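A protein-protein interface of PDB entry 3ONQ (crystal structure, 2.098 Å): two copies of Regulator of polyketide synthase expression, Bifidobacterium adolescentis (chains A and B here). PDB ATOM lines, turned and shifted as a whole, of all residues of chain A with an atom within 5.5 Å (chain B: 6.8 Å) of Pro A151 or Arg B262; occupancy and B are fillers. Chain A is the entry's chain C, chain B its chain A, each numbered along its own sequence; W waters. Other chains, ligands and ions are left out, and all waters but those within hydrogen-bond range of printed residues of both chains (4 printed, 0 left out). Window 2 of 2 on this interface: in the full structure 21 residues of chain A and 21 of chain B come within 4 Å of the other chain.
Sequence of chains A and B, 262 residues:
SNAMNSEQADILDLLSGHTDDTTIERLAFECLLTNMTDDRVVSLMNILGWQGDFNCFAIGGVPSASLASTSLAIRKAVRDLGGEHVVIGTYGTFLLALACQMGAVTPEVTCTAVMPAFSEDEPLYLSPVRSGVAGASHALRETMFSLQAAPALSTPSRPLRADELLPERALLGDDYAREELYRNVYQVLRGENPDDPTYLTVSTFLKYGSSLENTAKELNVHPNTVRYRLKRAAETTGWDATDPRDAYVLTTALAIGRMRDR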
ATOM      1  N   THR A  93       0.997  27.054 -27.051  1.00  0.00           N
ATOM      2  CA  THR A  93       2.358  27.397 -27.477  1.00  0.00           C
ATOM      3  C   THR A  93       2.575  27.154 -28.967  1.00  0.00           C
ATOM      4  O   THR A  93       3.642  27.475 -29.501  1.00  0.00           O
ATOM      5  CB  THR A  93       3.401  26.553 -26.733  1.00  0.00           C
ATOM      6  OG1 THR A  93       3.012  25.175 -26.793  1.00  0.00           O
ATOM      7  CG2 THR A  93       3.495  26.983 -25.276  1.00  0.00           C
ATOM      8  N   SER A 146      -3.341  16.648 -32.902  1.00  0.00           N
ATOM      9  CA  SER A 146      -2.152  15.813 -33.012  1.00  0.00           C
ATOM     10  C   SER A 146      -1.007  16.372 -32.182  1.00  0.00           C
ATOM     11  O   SER A 146      -0.273  15.617 -31.550  1.00  0.00           O
ATOM     12  CB  SER A 146      -1.710  15.631 -34.469  1.00  0.00           C
ATOM     13  OG  SER A 146      -2.663  14.868 -35.201  1.00  0.00           O
ATOM     14  N   LEU A 147      -0.841  17.691 -32.210  1.00  0.00           N
ATOM     15  CA  LEU A 147       0.196  18.350 -31.430  1.00  0.00           C
ATOM     16  C   LEU A 147      -0.052  18.185 -29.923  1.00  0.00           C
ATOM     17  O   LEU A 147       0.885  17.958 -29.161  1.00  0.00           O
ATOM     18  CB  LEU A 147       0.293  19.841 -31.811  1.00  0.00           C
ATOM     19  CG  LEU A 147       0.863  20.117 -33.214  1.00  0.00           C
ATOM     20  CD1 LEU A 147       0.782  21.592 -33.554  1.00  0.00           C
ATOM     21  CD2 LEU A 147       2.304  19.643 -33.301  1.00  0.00           C
ATOM     22  N   GLN A 148      -1.309  18.300 -29.495  1.00  0.00           N
ATOM     23  CA  GLN A 148      -1.650  18.059 -28.095  1.00  0.00           C
ATOM     24  C   GLN A 148      -1.385  16.613 -27.697  1.00  0.00           C
ATOM     25  O   GLN A 148      -1.110  16.335 -26.541  1.00  0.00           O
ATOM     26  CB  GLN A 148      -3.126  18.313 -27.829  1.00  0.00           C
ATOM     27  CG  GLN A 148      -3.562  19.740 -27.796  1.00  0.00           C
ATOM     28  CD  GLN A 148      -5.067  19.824 -27.611  1.00  0.00           C
ATOM     29  OE1 GLN A 148      -5.795  20.062 -28.565  1.00  0.00           O
ATOM     30  NE2 GLN A 148      -5.540  19.588 -26.385  1.00  0.00           N
ATOM     31  N   ALA A 149      -1.481  15.696 -28.655  1.00  0.00           N
ATOM     32  CA  ALA A 149      -1.416  14.276 -28.334  1.00  0.00           C
ATOM     33  C   ALA A 149       0.011  13.744 -28.380  1.00  0.00           C
ATOM     34  O   ALA A 149       0.316  12.696 -27.795  1.00  0.00           O
ATOM     35  CB  ALA A 149      -2.317  13.485 -29.278  1.00  0.00           C
ATOM     36  N   ALA A 150       0.874  14.483 -29.075  1.00  0.00           N
ATOM     37  CA  ALA A 150       2.251  14.062 -29.336  1.00  0.00           C
ATOM     38  C   ALA A 150       3.038  13.583 -28.111  1.00  0.00           C
ATOM     39  O   ALA A 150       3.831  12.652 -28.221  1.00  0.00           O
ATOM     40  CB  ALA A 150       3.032  15.174 -30.060  1.00  0.00           C
ATOM     41  N   PRO A 151       2.850  14.231 -26.949  1.00  0.00           N
ATOM     42  CA  PRO A 151       3.649  13.785 -25.792  1.00  0.00           C
ATOM     43  C   PRO A 151       3.414  12.315 -25.427  1.00  0.00           C
ATOM     44  O   PRO A 151       4.290  11.695 -24.816  1.00  0.00           O
ATOM     45  CB  PRO A 151       3.175  14.704 -24.663  1.00  0.00           C
ATOM     46  CG  PRO A 151       2.697  15.949 -25.365  1.00  0.00           C
ATOM     47  CD  PRO A 151       2.063  15.441 -26.645  1.00  0.00           C
ATOM     48  N   ALA A 152       2.283  11.752 -25.815  1.00  0.00           N
ATOM     49  CA  ALA A 152       2.014  10.348 -25.558  1.00  0.00           C
ATOM     50  C   ALA A 152       3.013   9.446 -26.275  1.00  0.00           C
ATOM     51  O   ALA A 152       3.309   8.371 -25.810  1.00  0.00           O
ATOM     52  CB  ALA A 152       0.600   9.982 -25.920  1.00  0.00           C
ATOM     53  N   LEU A 153       3.484   9.873 -27.438  1.00  0.00           N
ATOM     54  CA  LEU A 153       4.394   9.068 -28.242  1.00  0.00           C
ATOM     55  C   LEU A 153       5.829   8.992 -27.728  1.00  0.00           C
ATOM     56  O   LEU A 153       6.441   9.993 -27.409  1.00  0.00           O
ATOM     57  CB  LEU A 153       4.411   9.578 -29.673  1.00  0.00           C
ATOM     58  CG  LEU A 153       3.177   9.266 -30.501  1.00  0.00           C
ATOM     59  CD1 LEU A 153       3.424   9.547 -31.950  1.00  0.00           C
ATOM     60  CD2 LEU A 153       2.774   7.840 -30.303  1.00  0.00           C
ATOM     61  N   SER A 154       6.340   7.773 -27.637  1.00  0.00           N
ATOM     62  CA  SER A 154       7.720   7.527 -27.246  1.00  0.00           C
ATOM     63  C   SER A 154       8.767   7.974 -28.256  1.00  0.00           C
ATOM     64  O   SER A 154       9.716   8.668 -27.915  1.00  0.00           O
ATOM     65  CB  SER A 154       7.887   6.032 -26.989  1.00  0.00           C
ATOM     66  OG  SER A 154       6.626   5.380 -26.975  1.00  0.00           O
ATOM     67  N   LEU B 254      -1.209   6.353 -19.087  1.00  0.00           N
ATOM     68  CA  LEU B 254       0.075   7.007 -19.349  1.00  0.00           C
ATOM     69  C   LEU B 254      -0.034   8.084 -20.427  1.00  0.00           C
ATOM     70  O   LEU B 254       0.575   9.155 -20.297  1.00  0.00           O
ATOM     71  CB  LEU B 254       1.173   6.005 -19.703  1.00  0.00           C
ATOM     72  CG  LEU B 254       1.700   5.071 -18.597  1.00  0.00           C
ATOM     73  CD1 LEU B 254       3.094   4.558 -18.941  1.00  0.00           C
ATOM     74  CD2 LEU B 254       1.739   5.783 -17.284  1.00  0.00           C
ATOM     75  N   ALA B 255      -0.807   7.805 -21.482  1.00  0.00           N
ATOM     76  CA  ALA B 255      -1.042   8.787 -22.540  1.00  0.00           C
ATOM     77  C   ALA B 255      -1.746  10.013 -21.967  1.00  0.00           C
ATOM     78  O   ALA B 255      -1.369  11.162 -22.230  1.00  0.00           O
ATOM     79  CB  ALA B 255      -1.885   8.185 -23.669  1.00  0.00           C
ATOM     80  N   GLY B 257      -1.822  11.054 -18.861  1.00  0.00           N
ATOM     81  CA  GLY B 257      -0.938  11.788 -17.975  1.00  0.00           C
ATOM     82  C   GLY B 257       0.076  12.622 -18.740  1.00  0.00           C
ATOM     83  O   GLY B 257       0.294  13.794 -18.433  1.00  0.00           O
ATOM     84  N   ARG B 258       0.687  12.020 -19.750  1.00  0.00           N
ATOM     85  CA  ARG B 258       1.696  12.708 -20.554  1.00  0.00           C
ATOM     86  C   ARG B 258       1.149  13.914 -21.317  1.00  0.00           C
ATOM     87  O   ARG B 258       1.792  14.964 -21.367  1.00  0.00           O
ATOM     88  CB  ARG B 258       2.384  11.717 -21.496  1.00  0.00           C
ATOM     89  CG  ARG B 258       3.318  10.789 -20.725  1.00  0.00           C
ATOM     90  CD  ARG B 258       3.933   9.668 -21.557  1.00  0.00           C
ATOM     91  NE  ARG B 258       5.009   9.039 -20.788  1.00  0.00           N
ATOM     92  CZ  ARG B 258       5.288   7.737 -20.761  1.00  0.00           C
ATOM     93  NH1 ARG B 258       4.578   6.871 -21.479  1.00  0.00           N
ATOM     94  NH2 ARG B 258       6.287   7.297 -20.005  1.00  0.00           N
ATOM     95  N   MET B 259      -0.035  13.774 -21.906  1.00  0.00           N
ATOM     96  CA  MET B 259      -0.603  14.865 -22.673  1.00  0.00           C
ATOM     97  C   MET B 259      -0.968  15.982 -21.704  1.00  0.00           C
ATOM     98  O   MET B 259      -0.854  17.162 -22.020  1.00  0.00           O
ATOM     99  CB  MET B 259      -1.848  14.400 -23.426  1.00  0.00           C
ATOM    100  CG  MET B 259      -1.580  13.301 -24.440  1.00  0.00           C
ATOM    101  SD  MET B 259      -3.197  12.929 -25.484  1.00  0.00           S
ATOM    102  CE  MET B 259      -4.231  11.942 -24.153  1.00  0.00           C
ATOM    103  N   ARG B 260      -1.424  15.605 -20.520  1.00  0.00           N
ATOM    104  CA  ARG B 260      -1.850  16.598 -19.550  1.00  0.00           C
ATOM    105  C   ARG B 260      -0.668  17.332 -18.908  1.00  0.00           C
ATOM    106  O   ARG B 260      -0.723  18.542 -18.696  1.00  0.00           O
ATOM    107  CB  ARG B 260      -2.725  15.967 -18.479  1.00  0.00           C
ATOM    108  CG  ARG B 260      -3.238  16.972 -17.470  1.00  0.00           C
ATOM    109  CD  ARG B 260      -4.462  16.458 -16.764  1.00  0.00           C
ATOM    110  NE  ARG B 260      -4.776  17.270 -15.593  1.00  0.00           N
ATOM    111  CZ  ARG B 260      -5.829  17.057 -14.813  1.00  0.00           C
ATOM    112  NH1 ARG B 260      -6.662  16.064 -15.094  1.00  0.00           N
ATOM    113  NH2 ARG B 260      -6.055  17.838 -13.762  1.00  0.00           N
ATOM    114  N   ASP B 261       0.403  16.610 -18.606  1.00  0.00           N
ATOM    115  CA  ASP B 261       1.520  17.220 -17.885  1.00  0.00           C
ATOM    116  C   ASP B 261       2.505  17.941 -18.798  1.00  0.00           C
ATOM    117  O   ASP B 261       3.494  18.479 -18.315  1.00  0.00           O
ATOM    118  CB  ASP B 261       2.264  16.198 -17.028  1.00  0.00           C
ATOM    119  CG  ASP B 261       1.478  15.775 -15.815  1.00  0.00           C
ATOM    120  OD1 ASP B 261       0.426  16.387 -15.537  1.00  0.00           O
ATOM    121  OD2 ASP B 261       1.914  14.826 -15.139  1.00  0.00           O
ATOM    122  N   ARG B 262       2.245  17.927 -20.104  1.00  0.00           N
ATOM    123  CA  ARG B 262       2.921  18.825 -21.046  1.00  0.00           C
ATOM    124  C   ARG B 262       2.772  18.405 -22.498  1.00  0.00           C
ATOM    125  O   ARG B 262       3.329  19.046 -23.388  1.00  0.00           O
ATOM    126  CB  ARG B 262       4.403  18.998 -20.714  1.00  0.00           C
ATOM    127  CG  ARG B 262       4.893  20.416 -20.941  1.00  0.00           C
ATOM    128  CD  ARG B 262       3.902  21.421 -20.358  1.00  0.00           C
ATOM    129  NE  ARG B 262       4.331  22.806 -20.550  1.00  0.00           N
ATOM    130  CZ  ARG B 262       3.901  23.602 -21.527  1.00  0.00           C
ATOM    131  NH1 ARG B 262       3.017  23.157 -22.413  1.00  0.00           N
ATOM    132  NH2 ARG B 262       4.353  24.846 -21.619  1.00  0.00           N
HETATM  133  O   HOH W   1       1.756  19.015 -26.405  1.00  0.00           O
HETATM  134  O   HOH W   2      -0.849  18.063 -24.586  1.00  0.00           O
HETATM  135  O   HOH W   3       2.405   7.450 -23.321  1.00  0.00           O
HETATM  136  O   HOH W   4       5.976   8.257 -24.297  1.00  0.00           O
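Pro A151 touches just these residues of chain B: Arg B258 and Arg B262. Printed residues of chain A within 4 Å of Arg B262: Pro A151. Printed residues of chain B within 4 Å of Gln A148: Met B259 (3.7 Å). Printed residues of chain B within 4 Å of Ala A149: Met B259. Of the printed residues of chain A, Ala B255 touches Ala A152 (3.8 Å). The nearest residue of chain A that does not touch Arg B262 is Thr A93 (4.3 Å).
Gln A148 touches Met B259 (O to CG, 3.7 Å). Met B259 touches Ala A149. Pro A151 touches Arg B258. Pro A151 touches Arg B262. CB of Ala A152 touches CB of Ala B255, 3.8 Å away.
Of the 8 printed residues of chain B, 4 touch a printed residue of chain A. Hydrophobic or aromatic side chains of chain B that line the printed part of chain A: Ala B255 and Met B259. Hydrophobic or aromatic side chains of chain A within 4 Å of the printed part of chain B: Ala A149, Pro A151 and Ala A152. Among the printed residues, no Asp or Glu carboxylate lies within 4 Å of a Lys or Arg side-chain nitrogen of the other chain.
No position is printed for both chains.
Water W2 lies within hydrogen-bond range of the backbone carbonyl oxygen of Gln A148 (2.6 Å) and the backbone carbonyl oxygen of Met B259 (2.7 Å). Water W3 lies within hydrogen-bond range of O of Ala A152 (2.8 Å) and NH1 of Arg B258 (2.9 Å). Water W4 lies within hydrogen-bond range of O of Ala A152 (3.1 Å), N of Ser A154 (3.4 Å) and NH1 of Arg B258 (3.4 Å). Water W1 bridges the backbone carbonyl oxygen (O) of Leu A147 (3.1 Å) and the backbone carbonyl oxygen (O) of Arg B262 (3.4 Å).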
